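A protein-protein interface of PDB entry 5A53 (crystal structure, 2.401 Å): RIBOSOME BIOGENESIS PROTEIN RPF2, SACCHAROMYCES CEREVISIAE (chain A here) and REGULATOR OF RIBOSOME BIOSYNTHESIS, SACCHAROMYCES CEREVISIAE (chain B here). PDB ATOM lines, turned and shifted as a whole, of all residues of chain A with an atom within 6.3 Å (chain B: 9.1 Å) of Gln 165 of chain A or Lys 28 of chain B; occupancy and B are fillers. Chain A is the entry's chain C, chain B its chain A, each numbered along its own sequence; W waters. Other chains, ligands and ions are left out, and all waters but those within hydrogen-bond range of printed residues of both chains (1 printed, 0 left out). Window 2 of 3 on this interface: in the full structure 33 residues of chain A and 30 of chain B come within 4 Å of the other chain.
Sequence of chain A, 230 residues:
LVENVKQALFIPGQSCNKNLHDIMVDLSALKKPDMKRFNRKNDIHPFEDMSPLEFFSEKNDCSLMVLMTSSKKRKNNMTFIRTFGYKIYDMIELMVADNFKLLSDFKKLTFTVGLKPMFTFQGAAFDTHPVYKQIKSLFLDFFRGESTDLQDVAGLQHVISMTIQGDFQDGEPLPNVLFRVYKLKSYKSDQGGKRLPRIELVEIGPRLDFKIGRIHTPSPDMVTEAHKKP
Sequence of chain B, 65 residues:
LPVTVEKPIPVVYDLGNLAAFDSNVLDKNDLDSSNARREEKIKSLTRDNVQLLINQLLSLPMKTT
NH1 of Arg 38 of chain B is in salt-bridge range of OD2 of Asp 209 of chain A, at 3.1 Å.
The side-chain carboxylate (OD2) of Asp 167 of chain A lies within hydrogen-bond range of the backbone NH (N) of Leu 26 of chain B (3.1 Å).
The guanidinium group (NH2) of Arg 38 of chain B is in hydrogen-bond range of the side-chain amide oxygen (OE1) of Gln 165 of chain A.
O of Leu 31 of chain B sits at hydrogen-bond distance from NE of Arg 38 of chain B, 2.8 Å away.
The side-chain hydroxyl (OG) of Ser 34 of chain B lies within hydrogen-bond range of the side-chain carboxylate (OD2) of Asp 32 of chain B (2.5 Å).
The backbone carbonyl oxygen (O) of Asp 32 of chain B sits close to the guanidinium group (NE) of Arg 38 of chain B (3.3 Å).
NZ of Lys 28 of chain B is in salt-bridge range of OD1 of Asp 32 of chain B, 3.2 Å away.
NE2 of Gln 122 of chain A sits at hydrogen-bond distance from OG1 of Thr 163 of chain A (2.7 Å).
O of Thr 163 of chain A sits at hydrogen-bond distance from N of Leu 178 of chain A, 2.7 Å away.
Printed residues of chain B within 4 Å of Gln 122 of chain A: Leu 26.
Of the printed residues of chain B, Gln 165 of chain A touches Lys 28 (3.5 Å), Leu 31 (3.4 Å), Asp 32 (3.7 Å) and Arg 38 (3.3 Å).
Asn 176 of chain A touches none of the printed residues of chain B.
Printed residues of chain B within 4 Å of Leu 178 of chain A: Arg 38 and Ile 42.
Of chain A, only Gln 165 (3.5 Å) and Gly 166 (3.8 Å) come within 4 Å of Lys 28 of chain B.
Of the printed residues of chain A, Leu 31 of chain B touches Ile 164 (3.5 Å), Gln 165 (3.4 Å) and Gly 166 (3.5 Å).
Printed residues of chain A within 4 Å of Arg 38 of chain B: Gln 165, Leu 178 and Asp 209.
The nearest printed residue of chain B that does not touch Gln 165 of chain A is Ser 33 of chain B (4.01 Å).
The nearest printed residue of chain B that does not touch Leu 178 of chain A is Leu 31 of chain B (4.4 Å).
CD1 of Leu 26 of chain B touches O of Gln 122 of chain A (3.6 Å).
Ile 164 of chain A touches Leu 26 of chain B.
NE2 of Gln 165 of chain A touches CE of Lys 28 of chain B (3.5 Å).
Leu 31 of chain B touches Gln 165 of chain A (O to CG, 3.4 Å).
Gly 166 of chain A touches Leu 26 of chain B.
Gly 166 of chain A touches Lys 28 of chain B.
Leu 31 of chain B touches Gly 166 of chain A (CD1 to N, 3.5 Å).
Val 25 of chain B touches Asp 167 of chain A.
Arg 38 of chain B touches Leu 178 of chain A.
Ile 42 of chain B touches Leu 178 of chain A (CD1 to CD1, 3.6 Å).
Of the 11 printed residues of chain A, 7 touch a printed residue of chain B.
Hydrophobic or aromatic side chains of chain B that line the printed part of chain A: Val 25, Leu 26, Leu 31 and Ile 42.
Water W1 lies within hydrogen-bond range of OE1 of Gln 165 of chain A, ND2 of Asn 176 of chain A, OD2 of Asp 209 of chain A and NH2 of Arg 38 of chain B.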
ATOM      1  N   GLN A 122      16.553  10.640  11.983  1.00  0.00           N
ATOM      2  CA  GLN A 122      17.852  11.088  12.476  1.00  0.00           C
ATOM      3  C   GLN A 122      18.792   9.910  12.706  1.00  0.00           C
ATOM      4  O   GLN A 122      18.513   9.028  13.520  1.00  0.00           O
ATOM      5  CB  GLN A 122      17.694  11.892  13.770  1.00  0.00           C
ATOM      6  CG  GLN A 122      17.088  13.274  13.585  1.00  0.00           C
ATOM      7  CD  GLN A 122      15.575  13.245  13.482  1.00  0.00           C
ATOM      8  OE1 GLN A 122      15.007  13.591  12.448  1.00  0.00           O
ATOM      9  NE2 GLN A 122      14.917  12.833  14.557  1.00  0.00           N
ATOM     10  N   THR A 163      14.631   8.437  15.719  1.00  0.00           N
ATOM     11  CA  THR A 163      16.024   8.755  16.006  1.00  0.00           C
ATOM     12  C   THR A 163      16.767   7.558  16.585  1.00  0.00           C
ATOM     13  O   THR A 163      16.291   6.917  17.522  1.00  0.00           O
ATOM     14  CB  THR A 163      16.134   9.937  16.994  1.00  0.00           C
ATOM     15  OG1 THR A 163      15.379  11.050  16.500  1.00  0.00           O
ATOM     16  CG2 THR A 163      17.586  10.352  17.184  1.00  0.00           C
ATOM     17  N   ILE A 164      17.932   7.258  16.023  1.00  0.00           N
ATOM     18  CA  ILE A 164      18.790   6.215  16.567  1.00  0.00           C
ATOM     19  C   ILE A 164      19.472   6.734  17.829  1.00  0.00           C
ATOM     20  O   ILE A 164      20.019   7.835  17.836  1.00  0.00           O
ATOM     21  CB  ILE A 164      19.853   5.759  15.552  1.00  0.00           C
ATOM     22  CG1 ILE A 164      19.189   5.357  14.235  1.00  0.00           C
ATOM     23  CG2 ILE A 164      20.672   4.607  16.116  1.00  0.00           C
ATOM     24  CD1 ILE A 164      20.170   4.988  13.145  1.00  0.00           C
ATOM     25  N   GLN A 165      19.431   5.944  18.897  1.00  0.00           N
ATOM     26  CA  GLN A 165      19.988   6.374  20.174  1.00  0.00           C
ATOM     27  C   GLN A 165      21.513   6.413  20.124  1.00  0.00           C
ATOM     28  O   GLN A 165      22.187   5.510  20.622  1.00  0.00           O
ATOM     29  CB  GLN A 165      19.514   5.459  21.304  1.00  0.00           C
ATOM     30  CG  GLN A 165      19.616   6.086  22.688  1.00  0.00           C
ATOM     31  CD  GLN A 165      19.035   5.204  23.777  1.00  0.00           C
ATOM     32  OE1 GLN A 165      17.891   4.757  23.687  1.00  0.00           O
ATOM     33  NE2 GLN A 165      19.822   4.950  24.816  1.00  0.00           N
ATOM     34  N   GLY A 166      22.045   7.467  19.512  1.00  0.00           N
ATOM     35  CA  GLY A 166      23.478   7.672  19.428  1.00  0.00           C
ATOM     36  C   GLY A 166      24.140   6.900  18.305  1.00  0.00           C
ATOM     37  O   GLY A 166      23.660   5.842  17.895  1.00  0.00           O
ATOM     38  N   ASP A 167      25.247   7.435  17.800  1.00  0.00           N
ATOM     39  CA  ASP A 167      26.056   6.716  16.825  1.00  0.00           C
ATOM     40  C   ASP A 167      26.713   5.517  17.497  1.00  0.00           C
ATOM     41  O   ASP A 167      26.754   5.426  18.724  1.00  0.00           O
ATOM     42  CB  ASP A 167      27.112   7.633  16.203  1.00  0.00           C
ATOM     43  CG  ASP A 167      26.510   8.671  15.275  1.00  0.00           C
ATOM     44  OD1 ASP A 167      25.367   8.467  14.813  1.00  0.00           O
ATOM     45  OD2 ASP A 167      27.181   9.690  15.003  1.00  0.00           O
ATOM     46  N   PRO A 175      21.913   0.135  18.779  1.00  0.00           N
ATOM     47  CA  PRO A 175      21.184   1.135  19.569  1.00  0.00           C
ATOM     48  C   PRO A 175      19.684   1.129  19.283  1.00  0.00           C
ATOM     49  O   PRO A 175      19.267   0.804  18.171  1.00  0.00           O
ATOM     50  CB  PRO A 175      21.816   2.460  19.127  1.00  0.00           C
ATOM     51  CG  PRO A 175      23.174   2.086  18.639  1.00  0.00           C
ATOM     52  CD  PRO A 175      23.012   0.738  18.005  1.00  0.00           C
ATOM     53  N   ASN A 176      18.890   1.487  20.285  1.00  0.00           N
ATOM     54  CA  ASN A 176      17.442   1.563  20.131  1.00  0.00           C
ATOM     55  C   ASN A 176      17.018   2.644  19.141  1.00  0.00           C
ATOM     56  O   ASN A 176      17.779   3.564  18.845  1.00  0.00           O
ATOM     57  CB  ASN A 176      16.779   1.821  21.485  1.00  0.00           C
ATOM     58  CG  ASN A 176      16.883   0.634  22.426  1.00  0.00           C
ATOM     59  OD1 ASN A 176      17.460  -0.398  22.085  1.00  0.00           O
ATOM     60  ND2 ASN A 176      16.323   0.780  23.622  1.00  0.00           N
ATOM     61  N   VAL A 177      15.798   2.525  18.629  1.00  0.00           N
ATOM     62  CA  VAL A 177      15.231   3.553  17.767  1.00  0.00           C
ATOM     63  C   VAL A 177      14.119   4.288  18.508  1.00  0.00           C
ATOM     64  O   VAL A 177      13.201   3.666  19.044  1.00  0.00           O
ATOM     65  CB  VAL A 177      14.683   2.965  16.457  1.00  0.00           C
ATOM     66  CG1 VAL A 177      14.047   4.058  15.617  1.00  0.00           C
ATOM     67  CG2 VAL A 177      15.797   2.272  15.682  1.00  0.00           C
ATOM     68  N   LEU A 178      14.207   5.614  18.537  1.00  0.00           N
ATOM     69  CA  LEU A 178      13.309   6.423  19.354  1.00  0.00           C
ATOM     70  C   LEU A 178      12.152   7.004  18.542  1.00  0.00           C
ATOM     71  O   LEU A 178      12.319   7.964  17.791  1.00  0.00           O
ATOM     72  CB  LEU A 178      14.096   7.542  20.039  1.00  0.00           C
ATOM     73  CG  LEU A 178      15.381   7.079  20.738  1.00  0.00           C
ATOM     74  CD1 LEU A 178      16.065   8.230  21.450  1.00  0.00           C
ATOM     75  CD2 LEU A 178      15.098   5.942  21.708  1.00  0.00           C
ATOM     76  N   ASP A 209      10.375   3.607  22.742  1.00  0.00           N
ATOM     77  CA  ASP A 209      11.764   3.239  22.498  1.00  0.00           C
ATOM     78  C   ASP A 209      11.824   1.786  22.034  1.00  0.00           C
ATOM     79  O   ASP A 209      11.529   0.870  22.801  1.00  0.00           O
ATOM     80  CB  ASP A 209      12.615   3.437  23.755  1.00  0.00           C
ATOM     81  CG  ASP A 209      12.787   4.901  24.123  1.00  0.00           C
ATOM     82  OD1 ASP A 209      11.970   5.735  23.681  1.00  0.00           O
ATOM     83  OD2 ASP A 209      13.746   5.217  24.858  1.00  0.00           O
ATOM     84  N   VAL B  25      25.977  13.665  13.075  1.00  0.00           N
ATOM     85  CA  VAL B  25      26.441  12.898  14.226  1.00  0.00           C
ATOM     86  C   VAL B  25      25.499  12.998  15.423  1.00  0.00           C
ATOM     87  O   VAL B  25      25.058  14.087  15.793  1.00  0.00           O
ATOM     88  CB  VAL B  25      27.854  13.356  14.657  1.00  0.00           C
ATOM     89  CG1 VAL B  25      28.292  12.646  15.930  1.00  0.00           C
ATOM     90  CG2 VAL B  25      28.851  13.114  13.534  1.00  0.00           C
ATOM     91  N   LEU B  26      25.191  11.848  16.016  1.00  0.00           N
ATOM     92  CA  LEU B  26      24.370  11.779  17.217  1.00  0.00           C
ATOM     93  C   LEU B  26      25.211  11.351  18.415  1.00  0.00           C
ATOM     94  O   LEU B  26      26.053  10.459  18.303  1.00  0.00           O
ATOM     95  CB  LEU B  26      23.208  10.804  17.020  1.00  0.00           C
ATOM     96  CG  LEU B  26      22.198  11.151  15.926  1.00  0.00           C
ATOM     97  CD1 LEU B  26      21.289   9.967  15.638  1.00  0.00           C
ATOM     98  CD2 LEU B  26      21.385  12.364  16.331  1.00  0.00           C
ATOM     99  N   ASP B  27      24.983  11.984  19.562  1.00  0.00           N
ATOM    100  CA  ASP B  27      25.725  11.643  20.771  1.00  0.00           C
ATOM    101  C   ASP B  27      24.936  10.678  21.649  1.00  0.00           C
ATOM    102  O   ASP B  27      23.777  10.930  21.981  1.00  0.00           O
ATOM    103  CB  ASP B  27      26.079  12.903  21.563  1.00  0.00           C
ATOM    104  CG  ASP B  27      26.973  12.609  22.755  1.00  0.00           C
ATOM    105  OD1 ASP B  27      27.786  11.665  22.672  1.00  0.00           O
ATOM    106  OD2 ASP B  27      26.861  13.322  23.774  1.00  0.00           O
ATOM    107  N   LYS B  28      25.577   9.574  22.019  1.00  0.00           N
ATOM    108  CA  LYS B  28      24.951   8.550  22.848  1.00  0.00           C
ATOM    109  C   LYS B  28      24.520   9.098  24.208  1.00  0.00           C
ATOM    110  O   LYS B  28      23.434   8.787  24.696  1.00  0.00           O
ATOM    111  CB  LYS B  28      25.908   7.370  23.040  1.00  0.00           C
ATOM    112  CG  LYS B  28      25.442   6.346  24.064  1.00  0.00           C
ATOM    113  CD  LYS B  28      24.101   5.742  23.677  1.00  0.00           C
ATOM    114  CE  LYS B  28      23.281   5.392  24.908  1.00  0.00           C
ATOM    115  NZ  LYS B  28      23.864   4.244  25.653  1.00  0.00           N
ATOM    116  N   ASN B  29      25.376   9.916  24.810  1.00  0.00           N
ATOM    117  CA  ASN B  29      25.122  10.445  26.145  1.00  0.00           C
ATOM    118  C   ASN B  29      23.952  11.425  26.184  1.00  0.00           C
ATOM    119  O   ASN B  29      23.277  11.552  27.205  1.00  0.00           O
ATOM    120  CB  ASN B  29      26.384  11.116  26.691  1.00  0.00           C
ATOM    121  CG  ASN B  29      27.547  10.151  26.816  1.00  0.00           C
ATOM    122  OD1 ASN B  29      27.358   8.971  27.116  1.00  0.00           O
ATOM    123  ND2 ASN B  29      28.755  10.647  26.585  1.00  0.00           N
ATOM    124  N   ASP B  30      23.714  12.110  25.071  1.00  0.00           N
ATOM    125  CA  ASP B  30      22.605  13.057  24.983  1.00  0.00           C
ATOM    126  C   ASP B  30      21.257  12.346  24.899  1.00  0.00           C
ATOM    127  O   ASP B  30      20.221  12.926  25.225  1.00  0.00           O
ATOM    128  CB  ASP B  30      22.773  13.975  23.767  1.00  0.00           C
ATOM    129  CG  ASP B  30      23.869  15.005  23.956  1.00  0.00           C
ATOM    130  OD1 ASP B  30      24.050  15.481  25.096  1.00  0.00           O
ATOM    131  OD2 ASP B  30      24.543  15.347  22.962  1.00  0.00           O
ATOM    132  N   LEU B  31      21.274  11.088  24.469  1.00  0.00           N
ATOM    133  CA  LEU B  31      20.039  10.372  24.176  1.00  0.00           C
ATOM    134  C   LEU B  31      19.799   9.174  25.093  1.00  0.00           C
ATOM    135  O   LEU B  31      18.804   8.466  24.939  1.00  0.00           O
ATOM    136  CB  LEU B  31      20.041   9.905  22.719  1.00  0.00           C
ATOM    137  CG  LEU B  31      20.268  10.991  21.665  1.00  0.00           C
ATOM    138  CD1 LEU B  31      20.280  10.394  20.264  1.00  0.00           C
ATOM    139  CD2 LEU B  31      19.217  12.081  21.780  1.00  0.00           C
ATOM    140  N   ASP B  32      20.707   8.946  26.037  1.00  0.00           N
ATOM    141  CA  ASP B  32      20.573   7.827  26.966  1.00  0.00           C
ATOM    142  C   ASP B  32      19.315   7.978  27.817  1.00  0.00           C
ATOM    143  O   ASP B  32      18.913   9.091  28.152  1.00  0.00           O
ATOM    144  CB  ASP B  32      21.808   7.716  27.863  1.00  0.00           C
ATOM    145  CG  ASP B  32      21.804   6.453  28.706  1.00  0.00           C
ATOM    146  OD1 ASP B  32      22.315   5.418  28.229  1.00  0.00           O
ATOM    147  OD2 ASP B  32      21.289   6.496  29.843  1.00  0.00           O
ATOM    148  N   SER B  33      18.701   6.851  28.168  1.00  0.00           N
ATOM    149  CA  SER B  33      17.428   6.853  28.884  1.00  0.00           C
ATOM    150  C   SER B  33      17.532   7.437  30.292  1.00  0.00           C
ATOM    151  O   SER B  33      16.519   7.769  30.908  1.00  0.00           O
ATOM    152  CB  SER B  33      16.863   5.432  28.957  1.00  0.00           C
ATOM    153  OG  SER B  33      17.722   4.577  29.692  1.00  0.00           O
ATOM    154  N   SER B  34      18.755   7.562  30.800  1.00  0.00           N
ATOM    155  CA  SER B  34      18.972   8.116  32.131  1.00  0.00           C
ATOM    156  C   SER B  34      19.160   9.631  32.089  1.00  0.00           C
ATOM    157  O   SER B  34      18.989  10.313  33.099  1.00  0.00           O
ATOM    158  CB  SER B  34      20.179   7.451  32.798  1.00  0.00           C
ATOM    159  OG  SER B  34      21.352   7.624  32.023  1.00  0.00           O
ATOM    160  N   ASN B  35      19.513  10.152  30.916  1.00  0.00           N
ATOM    161  CA  ASN B  35      19.642  11.592  30.729  1.00  0.00           C
ATOM    162  C   ASN B  35      18.276  12.258  30.859  1.00  0.00           C
ATOM    163  O   ASN B  35      17.329  11.904  30.155  1.00  0.00           O
ATOM    164  CB  ASN B  35      20.274  11.904  29.368  1.00  0.00           C
ATOM    165  CG  ASN B  35      20.664  13.369  29.217  1.00  0.00           C
ATOM    166  OD1 ASN B  35      20.078  14.255  29.838  1.00  0.00           O
ATOM    167  ND2 ASN B  35      21.665  13.625  28.382  1.00  0.00           N
ATOM    168  N   ARG B  38      16.723  14.473  27.938  1.00  0.00           N
ATOM    169  CA  ARG B  38      16.566  13.625  26.760  1.00  0.00           C
ATOM    170  C   ARG B  38      15.596  14.187  25.728  1.00  0.00           C
ATOM    171  O   ARG B  38      15.985  14.531  24.612  1.00  0.00           O
ATOM    172  CB  ARG B  38      16.083  12.247  27.205  1.00  0.00           C
ATOM    173  CG  ARG B  38      16.468  11.087  26.317  1.00  0.00           C
ATOM    174  CD  ARG B  38      16.042   9.798  26.993  1.00  0.00           C
ATOM    175  NE  ARG B  38      16.259   8.618  26.165  1.00  0.00           N
ATOM    176  CZ  ARG B  38      15.303   7.751  25.854  1.00  0.00           C
ATOM    177  NH1 ARG B  38      14.068   7.939  26.301  1.00  0.00           N
ATOM    178  NH2 ARG B  38      15.580   6.698  25.098  1.00  0.00           N
ATOM    179  N   GLU B  39      14.329  14.265  26.118  1.00  0.00           N
ATOM    180  CA  GLU B  39      13.254  14.642  25.209  1.00  0.00           C
ATOM    181  C   GLU B  39      13.384  16.071  24.702  1.00  0.00           C
ATOM    182  O   GLU B  39      12.812  16.417  23.668  1.00  0.00           O
ATOM    183  CB  GLU B  39      11.898  14.453  25.893  1.00  0.00           C
ATOM    184  CG  GLU B  39      11.636  13.025  26.351  1.00  0.00           C
ATOM    185  CD  GLU B  39      11.602  12.035  25.199  1.00  0.00           C
ATOM    186  OE1 GLU B  39      11.201  12.427  24.082  1.00  0.00           O
ATOM    187  OE2 GLU B  39      11.980  10.864  25.409  1.00  0.00           O
ATOM    188  N   ILE B  42      15.646  15.472  21.667  1.00  0.00           N
ATOM    189  CA  ILE B  42      14.915  14.801  20.597  1.00  0.00           C
ATOM    190  C   ILE B  42      14.056  15.796  19.825  1.00  0.00           C
ATOM    191  O   ILE B  42      14.100  15.848  18.596  1.00  0.00           O
ATOM    192  CB  ILE B  42      14.001  13.679  21.132  1.00  0.00           C
ATOM    193  CG1 ILE B  42      14.710  12.868  22.217  1.00  0.00           C
ATOM    194  CG2 ILE B  42      13.524  12.786  19.988  1.00  0.00           C
ATOM    195  CD1 ILE B  42      15.631  11.812  21.683  1.00  0.00           C
HETATM  196  O   HOH W   1      15.995   3.241  25.033  1.00  0.00           O
